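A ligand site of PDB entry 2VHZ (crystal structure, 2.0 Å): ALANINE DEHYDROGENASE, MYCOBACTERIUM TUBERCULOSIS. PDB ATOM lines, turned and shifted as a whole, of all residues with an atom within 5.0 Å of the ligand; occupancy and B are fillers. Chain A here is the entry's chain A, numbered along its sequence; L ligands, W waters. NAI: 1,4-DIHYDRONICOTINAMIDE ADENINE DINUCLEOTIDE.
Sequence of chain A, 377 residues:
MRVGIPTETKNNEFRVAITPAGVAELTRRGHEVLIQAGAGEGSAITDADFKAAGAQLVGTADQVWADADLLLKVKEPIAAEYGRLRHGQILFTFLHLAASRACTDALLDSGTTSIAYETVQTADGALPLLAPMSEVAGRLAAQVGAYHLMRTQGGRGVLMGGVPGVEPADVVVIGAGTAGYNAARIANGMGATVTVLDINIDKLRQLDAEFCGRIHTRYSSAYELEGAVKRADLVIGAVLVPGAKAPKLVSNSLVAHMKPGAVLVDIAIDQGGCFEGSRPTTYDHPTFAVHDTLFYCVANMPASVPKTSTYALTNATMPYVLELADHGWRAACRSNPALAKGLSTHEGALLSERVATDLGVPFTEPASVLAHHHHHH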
ATOM      1  N   HIS A  96       6.941  12.270  17.222  1.00  0.00           N
ATOM      2  CA  HIS A  96       6.670  13.325  16.228  1.00  0.00           C
ATOM      3  C   HIS A  96       5.835  14.490  16.837  1.00  0.00           C
ATOM      4  O   HIS A  96       4.896  14.980  16.217  1.00  0.00           O
ATOM      5  CB  HIS A  96       5.978  12.752  14.982  1.00  0.00           C
ATOM      6  CG  HIS A  96       6.575  11.481  14.471  1.00  0.00           C
ATOM      7  ND1 HIS A  96       7.837  11.417  13.909  1.00  0.00           N
ATOM      8  CD2 HIS A  96       6.078  10.223  14.404  1.00  0.00           C
ATOM      9  CE1 HIS A  96       8.091  10.176  13.545  1.00  0.00           C
ATOM     10  NE2 HIS A  96       7.027   9.436  13.812  1.00  0.00           N
ATOM     11  N   LEU A 130      15.806   6.493  14.573  1.00  0.00           N
ATOM     12  CA  LEU A 130      15.158   6.967  13.340  1.00  0.00           C
ATOM     13  C   LEU A 130      15.799   6.353  12.081  1.00  0.00           C
ATOM     14  O   LEU A 130      15.091   5.938  11.155  1.00  0.00           O
ATOM     15  CB  LEU A 130      15.201   8.502  13.258  1.00  0.00           C
ATOM     16  CG  LEU A 130      14.515   9.051  12.005  1.00  0.00           C
ATOM     17  CD1 LEU A 130      13.014   8.678  11.982  1.00  0.00           C
ATOM     18  CD2 LEU A 130      14.729  10.567  11.874  1.00  0.00           C
ATOM     19  N   MET A 133      14.404   3.343  10.073  1.00  0.00           N
ATOM     20  CA  MET A 133      13.097   3.605   9.501  1.00  0.00           C
ATOM     21  C   MET A 133      13.227   4.572   8.322  1.00  0.00           C
ATOM     22  O   MET A 133      12.531   4.421   7.310  1.00  0.00           O
ATOM     23  CB  MET A 133      12.112   4.126  10.565  1.00  0.00           C
ATOM     24  CG  MET A 133      11.764   3.076  11.668  1.00  0.00           C
ATOM     25  SD  MET A 133      11.135   1.515  11.050  1.00  0.00           S
ATOM     26  CE  MET A 133      12.584   0.468  10.834  1.00  0.00           C
ATOM     27  N   SER A 134      14.135   5.536   8.441  1.00  0.00           N
ATOM     28  CA  SER A 134      14.436   6.419   7.320  1.00  0.00           C
ATOM     29  C   SER A 134      14.992   5.617   6.125  1.00  0.00           C
ATOM     30  O   SER A 134      14.689   5.938   4.973  1.00  0.00           O
ATOM     31  CB  SER A 134      15.445   7.490   7.742  1.00  0.00           C
ATOM     32  OG  SER A 134      14.829   8.384   8.649  1.00  0.00           O
ATOM     33  N   ALA A 137      11.824   3.852   4.652  1.00  0.00           N
ATOM     34  CA  ALA A 137      10.975   4.836   4.018  1.00  0.00           C
ATOM     35  C   ALA A 137      11.598   5.389   2.726  1.00  0.00           C
ATOM     36  O   ALA A 137      10.906   5.581   1.718  1.00  0.00           O
ATOM     37  CB  ALA A 137      10.667   6.001   5.014  1.00  0.00           C
ATOM     38  N   ILE A 174      14.835  15.829  -2.238  1.00  0.00           N
ATOM     39  CA  ILE A 174      15.201  16.968  -1.427  1.00  0.00           C
ATOM     40  C   ILE A 174      15.596  16.453  -0.064  1.00  0.00           C
ATOM     41  O   ILE A 174      14.749  15.971   0.701  1.00  0.00           O
ATOM     42  CB  ILE A 174      14.036  18.004  -1.274  1.00  0.00           C
ATOM     43  CG1 ILE A 174      13.359  18.224  -2.633  1.00  0.00           C
ATOM     44  CG2 ILE A 174      14.568  19.306  -0.658  1.00  0.00           C
ATOM     45  CD1 ILE A 174      11.984  18.957  -2.573  1.00  0.00           C
ATOM     46  N   GLY A 175      16.889  16.593   0.229  1.00  0.00           N
ATOM     47  CA  GLY A 175      17.501  16.091   1.456  1.00  0.00           C
ATOM     48  C   GLY A 175      18.404  14.932   1.077  1.00  0.00           C
ATOM     49  O   GLY A 175      17.952  13.973   0.448  1.00  0.00           O
ATOM     50  N   ALA A 176      19.665  15.015   1.502  1.00  0.00           N
ATOM     51  CA  ALA A 176      20.681  14.013   1.202  1.00  0.00           C
ATOM     52  C   ALA A 176      21.057  13.222   2.457  1.00  0.00           C
ATOM     53  O   ALA A 176      22.194  12.781   2.602  1.00  0.00           O
ATOM     54  CB  ALA A 176      21.945  14.677   0.636  1.00  0.00           C
ATOM     55  N   GLY A 177      20.124  13.103   3.386  1.00  0.00           N
ATOM     56  CA  GLY A 177      20.376  12.379   4.617  1.00  0.00           C
ATOM     57  C   GLY A 177      20.013  10.926   4.403  1.00  0.00           C
ATOM     58  O   GLY A 177      20.024  10.426   3.270  1.00  0.00           O
ATOM     59  N   THR A 178      19.666  10.242   5.486  1.00  0.00           N
ATOM     60  CA  THR A 178      19.404   8.814   5.427  1.00  0.00           C
ATOM     61  C   THR A 178      18.287   8.451   4.437  1.00  0.00           C
ATOM     62  O   THR A 178      18.458   7.587   3.561  1.00  0.00           O
ATOM     63  CB  THR A 178      19.097   8.255   6.833  1.00  0.00           C
ATOM     64  OG1 THR A 178      20.197   8.584   7.706  1.00  0.00           O
ATOM     65  CG2 THR A 178      18.940   6.744   6.769  1.00  0.00           C
ATOM     66  N   ALA A 179      17.133   9.092   4.604  1.00  0.00           N
ATOM     67  CA  ALA A 179      15.990   8.795   3.727  1.00  0.00           C
ATOM     68  C   ALA A 179      16.265   9.191   2.266  1.00  0.00           C
ATOM     69  O   ALA A 179      15.946   8.429   1.344  1.00  0.00           O
ATOM     70  CB  ALA A 179      14.701   9.471   4.250  1.00  0.00           C
ATOM     71  N   GLY A 180      16.893  10.351   2.055  1.00  0.00           N
ATOM     72  CA  GLY A 180      17.104  10.847   0.683  1.00  0.00           C
ATOM     73  C   GLY A 180      18.139  10.026  -0.049  1.00  0.00           C
ATOM     74  O   GLY A 180      17.961   9.679  -1.220  1.00  0.00           O
ATOM     75  N   LEU A 197      19.135  17.341  -3.730  1.00  0.00           N
ATOM     76  CA  LEU A 197      19.494  18.658  -3.182  1.00  0.00           C
ATOM     77  C   LEU A 197      19.664  18.636  -1.680  1.00  0.00           C
ATOM     78  O   LEU A 197      18.977  17.885  -0.976  1.00  0.00           O
ATOM     79  CB  LEU A 197      18.429  19.710  -3.530  1.00  0.00           C
ATOM     80  CG  LEU A 197      18.314  19.915  -5.057  1.00  0.00           C
ATOM     81  CD1 LEU A 197      17.115  19.185  -5.635  1.00  0.00           C
ATOM     82  CD2 LEU A 197      18.275  21.354  -5.452  1.00  0.00           C
ATOM     83  N   ASP A 198      20.568  19.467  -1.176  1.00  0.00           N
ATOM     84  CA  ASP A 198      20.724  19.668   0.252  1.00  0.00           C
ATOM     85  C   ASP A 198      21.406  21.022   0.457  1.00  0.00           C
ATOM     86  O   ASP A 198      22.108  21.546  -0.425  1.00  0.00           O
ATOM     87  CB  ASP A 198      21.584  18.534   0.877  1.00  0.00           C
ATOM     88  CG  ASP A 198      21.266  18.287   2.372  1.00  0.00           C
ATOM     89  OD1 ASP A 198      21.423  19.229   3.192  1.00  0.00           O
ATOM     90  OD2 ASP A 198      20.867  17.129   2.732  1.00  0.00           O
ATOM     91  N   ILE A 199      21.210  21.571   1.645  1.00  0.00           N
ATOM     92  CA  ILE A 199      21.943  22.761   2.072  1.00  0.00           C
ATOM     93  C   ILE A 199      23.287  22.397   2.711  1.00  0.00           C
ATOM     94  O   ILE A 199      24.155  23.260   2.914  1.00  0.00           O
ATOM     95  CB  ILE A 199      21.110  23.647   3.016  1.00  0.00           C
ATOM     96  CG1 ILE A 199      20.543  22.829   4.169  1.00  0.00           C
ATOM     97  CG2 ILE A 199      20.020  24.368   2.219  1.00  0.00           C
ATOM     98  CD1 ILE A 199      19.933  23.705   5.281  1.00  0.00           C
ATOM     99  N   ASN A 200      23.466  21.115   3.029  1.00  0.00           N
ATOM    100  CA  ASN A 200      24.710  20.635   3.579  1.00  0.00           C
ATOM    101  C   ASN A 200      25.564  20.036   2.457  1.00  0.00           C
ATOM    102  O   ASN A 200      25.300  18.925   2.004  1.00  0.00           O
ATOM    103  CB  ASN A 200      24.467  19.573   4.673  1.00  0.00           C
ATOM    104  CG  ASN A 200      25.762  19.150   5.382  1.00  0.00           C
ATOM    105  OD1 ASN A 200      26.877  19.347   4.865  1.00  0.00           O
ATOM    106  ND2 ASN A 200      25.626  18.595   6.577  1.00  0.00           N
ATOM    107  N   LYS A 203      27.218  16.451   2.650  1.00  0.00           N
ATOM    108  CA  LYS A 203      26.352  15.348   2.283  1.00  0.00           C
ATOM    109  C   LYS A 203      26.284  15.145   0.770  1.00  0.00           C
ATOM    110  O   LYS A 203      26.238  14.021   0.292  1.00  0.00           O
ATOM    111  CB  LYS A 203      24.976  15.524   2.934  1.00  0.00           C
ATOM    112  CG  LYS A 203      25.021  14.901   4.361  1.00  0.00           C
ATOM    113  CD  LYS A 203      23.957  15.402   5.223  1.00  0.00           C
ATOM    114  CE  LYS A 203      23.841  14.499   6.445  1.00  0.00           C
ATOM    115  NZ  LYS A 203      22.635  14.875   7.224  1.00  0.00           N
ATOM    116  N   SER A 220      21.075  23.405  -2.524  1.00  0.00           N
ATOM    117  CA  SER A 220      19.660  23.713  -2.454  1.00  0.00           C
ATOM    118  C   SER A 220      19.403  25.221  -2.339  1.00  0.00           C
ATOM    119  O   SER A 220      18.897  25.692  -1.321  1.00  0.00           O
ATOM    120  CB  SER A 220      19.032  22.976  -1.288  1.00  0.00           C
ATOM    121  OG  SER A 220      17.638  22.897  -1.486  1.00  0.00           O
ATOM    122  N   ALA A 238      12.514  14.710   1.722  1.00  0.00           N
ATOM    123  CA  ALA A 238      13.206  13.930   2.739  1.00  0.00           C
ATOM    124  C   ALA A 238      14.089  14.787   3.646  1.00  0.00           C
ATOM    125  O   ALA A 238      15.214  14.366   4.012  1.00  0.00           O
ATOM    126  CB  ALA A 238      14.050  12.818   2.043  1.00  0.00           C
ATOM    127  N   VAL A 239      13.646  16.003   3.940  1.00  0.00           N
ATOM    128  CA  VAL A 239      14.436  16.889   4.792  1.00  0.00           C
ATOM    129  C   VAL A 239      14.054  16.691   6.245  1.00  0.00           C
ATOM    130  O   VAL A 239      12.969  16.149   6.544  1.00  0.00           O
ATOM    131  CB  VAL A 239      14.349  18.380   4.404  1.00  0.00           C
ATOM    132  CG1 VAL A 239      14.901  18.598   2.994  1.00  0.00           C
ATOM    133  CG2 VAL A 239      12.933  18.911   4.549  1.00  0.00           C
ATOM    134  N   LEU A 240      14.951  17.094   7.136  1.00  0.00           N
ATOM    135  CA  LEU A 240      14.718  16.974   8.572  1.00  0.00           C
ATOM    136  C   LEU A 240      15.597  17.977   9.291  1.00  0.00           C
ATOM    137  O   LEU A 240      16.771  18.149   8.942  1.00  0.00           O
ATOM    138  CB  LEU A 240      15.053  15.567   9.095  1.00  0.00           C
ATOM    139  CG  LEU A 240      14.939  15.330  10.621  1.00  0.00           C
ATOM    140  CD1 LEU A 240      13.488  15.488  11.201  1.00  0.00           C
ATOM    141  CD2 LEU A 240      15.554  13.978  11.048  1.00  0.00           C
ATOM    142  N   VAL A 241      15.009  18.648  10.270  1.00  0.00           N
ATOM    143  CA  VAL A 241      15.772  19.251  11.360  1.00  0.00           C
ATOM    144  C   VAL A 241      15.364  18.483  12.627  1.00  0.00           C
ATOM    145  O   VAL A 241      14.191  18.463  12.969  1.00  0.00           O
ATOM    146  CB  VAL A 241      15.474  20.737  11.491  1.00  0.00           C
ATOM    147  CG1 VAL A 241      16.125  21.308  12.758  1.00  0.00           C
ATOM    148  CG2 VAL A 241      15.951  21.494  10.213  1.00  0.00           C
ATOM    149  N   PRO A 247      10.484  22.122   7.530  1.00  0.00           N
ATOM    150  CA  PRO A 247      10.319  23.365   6.765  1.00  0.00           C
ATOM    151  C   PRO A 247       9.513  23.122   5.495  1.00  0.00           C
ATOM    152  O   PRO A 247       9.574  22.039   4.913  1.00  0.00           O
ATOM    153  CB  PRO A 247      11.760  23.751   6.415  1.00  0.00           C
ATOM    154  CG  PRO A 247      12.517  22.472   6.429  1.00  0.00           C
ATOM    155  CD  PRO A 247      11.886  21.663   7.534  1.00  0.00           C
ATOM    156  N   LEU A 249       9.227  23.600   1.889  1.00  0.00           N
ATOM    157  CA  LEU A 249      10.157  23.900   0.813  1.00  0.00           C
ATOM    158  C   LEU A 249       9.536  23.932  -0.588  1.00  0.00           C
ATOM    159  O   LEU A 249      10.082  24.573  -1.474  1.00  0.00           O
ATOM    160  CB  LEU A 249      11.341  22.899   0.843  1.00  0.00           C
ATOM    161  CG  LEU A 249      12.162  22.874   2.144  1.00  0.00           C
ATOM    162  CD1 LEU A 249      13.237  21.782   2.118  1.00  0.00           C
ATOM    163  CD2 LEU A 249      12.787  24.256   2.449  1.00  0.00           C
ATOM    164  N   ASP A 266       6.006  12.793   0.077  1.00  0.00           N
ATOM    165  CA  ASP A 266       6.476  13.582   1.205  1.00  0.00           C
ATOM    166  C   ASP A 266       6.833  12.645   2.341  1.00  0.00           C
ATOM    167  O   ASP A 266       5.971  12.259   3.143  1.00  0.00           O
ATOM    168  CB  ASP A 266       5.439  14.623   1.659  1.00  0.00           C
ATOM    169  CG  ASP A 266       6.079  15.770   2.490  1.00  0.00           C
ATOM    170  OD1 ASP A 266       7.195  15.601   3.015  1.00  0.00           O
ATOM    171  OD2 ASP A 266       5.460  16.844   2.608  1.00  0.00           O
ATOM    172  N   ILE A 267       8.103  12.251   2.416  1.00  0.00           N
ATOM    173  CA  ILE A 267       8.532  11.350   3.497  1.00  0.00           C
ATOM    174  C   ILE A 267       8.481  12.097   4.829  1.00  0.00           C
ATOM    175  O   ILE A 267       8.135  11.500   5.860  1.00  0.00           O
ATOM    176  CB  ILE A 267       9.967  10.797   3.288  1.00  0.00           C
ATOM    177  CG1 ILE A 267      10.113  10.103   1.920  1.00  0.00           C
ATOM    178  CG2 ILE A 267      10.332   9.818   4.438  1.00  0.00           C
ATOM    179  CD1 ILE A 267      11.528   9.475   1.675  1.00  0.00           C
ATOM    180  N   ALA A 268       8.777  13.396   4.786  1.00  0.00           N
ATOM    181  CA  ALA A 268       8.829  14.259   5.983  1.00  0.00           C
ATOM    182  C   ALA A 268       7.436  14.579   6.550  1.00  0.00           C
ATOM    183  O   ALA A 268       7.300  15.383   7.484  1.00  0.00           O
ATOM    184  CB  ALA A 268       9.587  15.550   5.672  1.00  0.00           C
ATOM    185  N   ILE A 269       6.389  13.985   5.977  1.00  0.00           N
ATOM    186  CA  ILE A 269       5.037  14.117   6.504  1.00  0.00           C
ATOM    187  C   ILE A 269       4.946  13.772   7.996  1.00  0.00           C
ATOM    188  O   ILE A 269       4.144  14.383   8.730  1.00  0.00           O
ATOM    189  CB  ILE A 269       3.986  13.308   5.663  1.00  0.00           C
ATOM    190  CG1 ILE A 269       2.533  13.646   6.111  1.00  0.00           C
ATOM    191  CG2 ILE A 269       4.236  11.807   5.796  1.00  0.00           C
ATOM    192  CD1 ILE A 269       2.123  15.103   5.965  1.00  0.00           C
ATOM    193  N   ASP A 270       5.766  12.831   8.475  1.00  0.00           N
ATOM    194  CA  ASP A 270       5.708  12.464   9.902  1.00  0.00           C
ATOM    195  C   ASP A 270       6.047  13.639  10.822  1.00  0.00           C
ATOM    196  O   ASP A 270       5.595  13.688  11.960  1.00  0.00           O
ATOM    197  CB  ASP A 270       6.587  11.241  10.216  1.00  0.00           C
ATOM    198  CG  ASP A 270       8.060  11.502   9.953  1.00  0.00           C
ATOM    199  OD1 ASP A 270       8.876  10.770  10.527  1.00  0.00           O
ATOM    200  OD2 ASP A 270       8.405  12.426   9.185  1.00  0.00           O
ATOM    201  N   GLN A 271       6.811  14.607  10.290  1.00  0.00           N
ATOM    202  CA  GLN A 271       7.167  15.807  11.025  1.00  0.00           C
ATOM    203  C   GLN A 271       6.385  17.029  10.545  1.00  0.00           C
ATOM    204  O   GLN A 271       6.776  18.169  10.833  1.00  0.00           O
ATOM    205  CB  GLN A 271       8.688  16.064  10.999  1.00  0.00           C
ATOM    206  CG  GLN A 271       9.533  14.945  11.665  1.00  0.00           C
ATOM    207  CD  GLN A 271       9.385  14.901  13.187  1.00  0.00           C
ATOM    208  OE1 GLN A 271       9.226  13.815  13.775  1.00  0.00           O
ATOM    209  NE2 GLN A 271       9.465  16.060  13.846  1.00  0.00           N
ATOM    210  N   VAL A 298       2.235   9.355   3.390  1.00  0.00           N
ATOM    211  CA  VAL A 298       1.997   8.332   4.417  1.00  0.00           C
ATOM    212  C   VAL A 298       3.016   8.466   5.548  1.00  0.00           C
ATOM    213  O   VAL A 298       4.224   8.380   5.308  1.00  0.00           O
ATOM    214  CB  VAL A 298       2.012   6.912   3.801  1.00  0.00           C
ATOM    215  CG1 VAL A 298       1.974   5.814   4.883  1.00  0.00           C
ATOM    216  CG2 VAL A 298       0.844   6.770   2.834  1.00  0.00           C
ATOM    217  N   ALA A 299       2.514   8.677   6.766  1.00  0.00           N
ATOM    218  CA  ALA A 299       3.372   8.930   7.951  1.00  0.00           C
ATOM    219  C   ALA A 299       3.862   7.657   8.645  1.00  0.00           C
ATOM    220  O   ALA A 299       4.598   7.738   9.642  1.00  0.00           O
ATOM    221  CB  ALA A 299       2.656   9.854   8.963  1.00  0.00           C
ATOM    222  N   ASN A 300       3.500   6.500   8.112  1.00  0.00           N
ATOM    223  CA  ASN A 300       4.004   5.237   8.654  1.00  0.00           C
ATOM    224  C   ASN A 300       4.399   4.277   7.546  1.00  0.00           C
ATOM    225  O   ASN A 300       4.013   3.097   7.547  1.00  0.00           O
ATOM    226  CB  ASN A 300       3.012   4.594   9.668  1.00  0.00           C
ATOM    227  CG  ASN A 300       1.727   4.048   9.021  1.00  0.00           C
ATOM    228  OD1 ASN A 300       1.263   4.584   8.023  1.00  0.00           O
ATOM    229  ND2 ASN A 300       1.149   2.983   9.621  1.00  0.00           N
ATOM    230  N   MET A 301       5.208   4.783   6.617  1.00  0.00           N
ATOM    231  CA  MET A 301       5.585   4.028   5.418  1.00  0.00           C
ATOM    232  C   MET A 301       6.143   2.641   5.747  1.00  0.00           C
ATOM    233  O   MET A 301       5.738   1.695   5.092  1.00  0.00           O
ATOM    234  CB  MET A 301       6.560   4.818   4.521  1.00  0.00           C
ATOM    235  CG  MET A 301       5.891   6.050   3.875  1.00  0.00           C
ATOM    236  SD  MET A 301       7.091   7.185   3.126  1.00  0.00           S
ATOM    237  CE  MET A 301       7.359   6.352   1.570  1.00  0.00           C
ATOM    238  N   PRO A 302       7.055   2.515   6.740  1.00  0.00           N
ATOM    239  CA  PRO A 302       7.634   1.163   6.963  1.00  0.00           C
ATOM    240  C   PRO A 302       6.659   0.065   7.383  1.00  0.00           C
ATOM    241  O   PRO A 302       7.024  -1.130   7.399  1.00  0.00           O
ATOM    242  CB  PRO A 302       8.693   1.411   8.061  1.00  0.00           C
ATOM    243  CG  PRO A 302       9.056   2.934   7.918  1.00  0.00           C
ATOM    244  CD  PRO A 302       7.662   3.510   7.655  1.00  0.00           C
HETATM  245  PA  NAI L   1      18.567  13.158   8.098  1.00  0.00           P
HETATM  246  O1A NAI L   1      18.809  14.107   9.210  1.00  0.00           O
HETATM  247  O2A NAI L   1      19.450  11.927   7.885  1.00  0.00           O
HETATM  248  O5B NAI L   1      18.547  14.014   6.731  1.00  0.00           O
HETATM  249  C5B NAI L   1      17.801  15.214   6.553  1.00  0.00           C
HETATM  250  C4B NAI L   1      18.528  16.082   5.514  1.00  0.00           C
HETATM  251  O4B NAI L   1      17.716  17.225   5.179  1.00  0.00           O
HETATM  252  C3B NAI L   1      19.845  16.637   6.086  1.00  0.00           C
HETATM  253  O3B NAI L   1      20.906  16.225   5.244  1.00  0.00           O
HETATM  254  C2B NAI L   1      19.670  18.159   6.076  1.00  0.00           C
HETATM  255  O2B NAI L   1      20.840  18.958   5.795  1.00  0.00           O
HETATM  256  C1B NAI L   1      18.600  18.320   5.016  1.00  0.00           C
HETATM  257  N9A NAI L   1      17.881  19.605   5.171  1.00  0.00           N
HETATM  258  C8A NAI L   1      17.430  20.178   6.319  1.00  0.00           C
HETATM  259  N7A NAI L   1      16.839  21.358   6.030  1.00  0.00           N
HETATM  260  C5A NAI L   1      16.916  21.540   4.696  1.00  0.00           C
HETATM  261  C6A NAI L   1      16.492  22.575   3.736  1.00  0.00           C
HETATM  262  N6A NAI L   1      15.850  23.684   4.193  1.00  0.00           N
HETATM  263  N1A NAI L   1      16.774  22.363   2.425  1.00  0.00           N
HETATM  264  C2A NAI L   1      17.423  21.265   1.961  1.00  0.00           C
HETATM  265  N3A NAI L   1      17.828  20.260   2.784  1.00  0.00           N
HETATM  266  C4A NAI L   1      17.598  20.365   4.122  1.00  0.00           C
HETATM  267  O3  NAI L   1      17.025  12.740   8.191  1.00  0.00           O
HETATM  268  PN  NAI L   1      16.354  11.422   7.657  1.00  0.00           P
HETATM  269  O1N NAI L   1      16.559  10.299   8.643  1.00  0.00           O
HETATM  270  O2N NAI L   1      16.651  11.179   6.203  1.00  0.00           O
HETATM  271  O5D NAI L   1      14.823  11.851   7.753  1.00  0.00           O
HETATM  272  C5D NAI L   1      14.114  12.671   6.816  1.00  0.00           C
HETATM  273  C4D NAI L   1      12.640  12.675   7.197  1.00  0.00           C
HETATM  274  O4D NAI L   1      12.066  11.376   6.941  1.00  0.00           O
HETATM  275  C3D NAI L   1      12.399  12.940   8.697  1.00  0.00           C
HETATM  276  O3D NAI L   1      11.248  13.795   8.916  1.00  0.00           O
HETATM  277  C2D NAI L   1      12.044  11.565   9.228  1.00  0.00           C
HETATM  278  O2D NAI L   1      11.361  11.634  10.495  1.00  0.00           O
HETATM  279  C1D NAI L   1      11.205  11.099   8.046  1.00  0.00           C
HETATM  280  N1N NAI L   1      10.758   9.704   8.090  1.00  0.00           N
HETATM  281  C2N NAI L   1       9.492   9.466   7.693  1.00  0.00           C
HETATM  282  C3N NAI L   1       8.962   8.169   7.698  1.00  0.00           C
HETATM  283  C7N NAI L   1       7.555   7.937   7.221  1.00  0.00           C
HETATM  284  O7N NAI L   1       7.029   6.858   7.480  1.00  0.00           O
HETATM  285  N7N NAI L   1       6.917   8.893   6.517  1.00  0.00           N
HETATM  286  C4N NAI L   1       9.775   7.103   8.131  1.00  0.00           C
HETATM  287  C5N NAI L   1      11.090   7.381   8.519  1.00  0.00           C
HETATM  288  C6N NAI L   1      11.575   8.692   8.494  1.00  0.00           C
HETATM  289  O   HOH W   1      19.037  16.735   9.582  1.00  0.00           O
HETATM  290  O   HOH W   2      16.108  23.785   7.200  1.00  0.00           O
HETATM  291  O   HOH W   3      11.206  16.540   8.730  1.00  0.00           O
HETATM  292  O   HOH W   4      16.220  24.124   0.490  1.00  0.00           O
HETATM  293  O   HOH W   5      22.947  18.212   7.563  1.00  0.00           O
HETATM  294  O   HOH W   6      21.967  12.040   7.792  1.00  0.00           O
HETATM  295  O   HOH W   7      11.769  12.618  13.074  1.00  0.00           O
HETATM  296  O   HOH W   8      18.760   9.249  10.095  1.00  0.00           O
HETATM  297  O   HOH W   9      17.198  12.625   3.946  1.00  0.00           O
HETATM  298  O   HOH W  10      20.567  13.777  11.555  1.00  0.00           O
HETATM  299  O   HOH W  11      21.859  20.920   7.511  1.00  0.00           O
HETATM  300  O   HOH W  12      15.865  26.265   2.620  1.00  0.00           O
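The side-chain hydroxyl (OG) of Ser 134 is in hydrogen-bond range of an oxygen (O1N) of the ligand, at 2.6 Å. The side-chain carboxylate (OD1) of Asp 270 sits at hydrogen-bond distance from an oxygen (O2D) of the ligand, at 2.6 Å. An oxygen (O3B) of the ligand is in hydrogen-bond range of the side-chain carboxylate of Asp 198 (2.7 Å). The backbone NH (N) of Ala 179 is in hydrogen-bond range of an oxygen (O2N) of the ligand. An oxygen (O7N) of the ligand sits at hydrogen-bond distance from the backbone NH of Met 301 (2.9 Å). The backbone NH of Thr 178 is in hydrogen-bond range of an oxygen (O2A) of the ligand (2.9 Å). OG1 of Thr 178 sits at hydrogen-bond distance from O2A of the ligand. N7N of the ligand sits at hydrogen-bond distance from O of Ile 267, at 3.0 Å. An oxygen (O3B) of the ligand is in hydrogen-bond range of the side-chain amino group (NZ) of Lys 203, at 3.0 Å. The backbone carbonyl oxygen (O) of Val 298 sits at hydrogen-bond distance from a nitrogen (N7N) of the ligand (3.0 Å). An oxygen (O4B) of the ligand sits at hydrogen-bond distance from the backbone NH (N) of Leu 240, at 3.4 Å.
The backbone carbonyl oxygen (O) of Asp 198 lies within hydrogen-bond range of the backbone NH (N) of Ser 220, 3.0 Å away. N of Asn 200 sits at hydrogen-bond distance from OD1 of Asp 198 (2.8 Å). The side-chain carboxylate (OD2) of Asp 198 sits at hydrogen-bond distance from the backbone NH (N) of Ala 176, 2.7 Å away. The backbone NH (N) of Val 239 lies within hydrogen-bond range of the backbone carbonyl oxygen (O) of Ile 174, 3.4 Å away. ND1 of His 96 is in hydrogen-bond range of OE1 of Gln 271, at 2.8 Å. N of Ala 238 lies within hydrogen-bond range of O of Ile 174. The backbone NH (N) of Ala 268 sits close to the side-chain carboxylate (OD1) of Asp 266. The backbone NH (N) of Gly 175 lies within hydrogen-bond range of the backbone carbonyl oxygen (O) of Leu 197 (2.7 Å).
The backbone carbonyl oxygen (O) of Ala 299 lies close to an oxygen (O7N) of the ligand (3.4 Å). CD1 of Leu 130 touches O2D of the ligand, at 3.7 Å. Met 133 touches the ligand. CB of Ala 137 touches C4N of the ligand, at 3.4 Å. CA of Gly 175 touches O4B of the ligand, 3.9 Å away. Gly 177 touches the ligand (CA to O5B, 3.2 Å). Ile 199 touches the ligand (CD1 to C5A, 3.8 Å). Asn 200 touches the ligand (CB to O2B, 3.8 Å). OG of Ser 220 touches C2A of the ligand, 3.8 Å away. Ala 238 touches the ligand. Val 239 touches the ligand (CA to O4B, 3.3 Å). Leu 249 touches the ligand. CA of Ala 268 touches O3D of the ligand, 3.8 Å away. Gln 271 touches the ligand (CG to O3D, 3.4 Å). Asn 300 touches the ligand (N to O7N, 3.6 Å). CD of Pro 302 touches O7N of the ligand, at 3.4 Å. Within 4 Å of the ligand: Leu 130, Met 133, Ser 134, Ala 137, Gly 175, Gly 177, Thr 178, Ala 179, Asp 198, Ile 199, Asn 200, Lys 203, Ser 220, Ala 238, Val 239, Leu 240, Leu 249, Ile 267, Ala 268, Asp 270, Gln 271, Val 298, Ala 299, Asn 300, Met 301 and Pro 302. The nearest printed residue that does not touch the ligand is Ile 269 (4.02 Å).
Water W6 bridges an oxygen (O2A) of the ligand (2.5 Å) and the side-chain amino group (NZ) of Lys 203 (3.0 Å). Water W4 lies within hydrogen-bond range of N1A of the ligand and OG of Ser 220. Water W9 lies within hydrogen-bond range of O of Ala 238 (2.6 Å), O2N of the ligand (2.7 Å), N of Gly 180 (3.0 Å) and N of Gly 177 (3.0 Å). Water W3 lies within hydrogen-bond range of an oxygen (O3D) of the ligand (2.8 Å) and the backbone carbonyl oxygen of Val 239 (2.8 Å). Water W8 lies within hydrogen-bond range of an oxygen (O1N) of the ligand and the side-chain hydroxyl (OG1) of Thr 178. Water W5 lies within hydrogen-bond range of an oxygen (O2B) of the ligand, the side-chain amide nitrogen of Asn 200 and the side-chain amino group of Lys 203.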
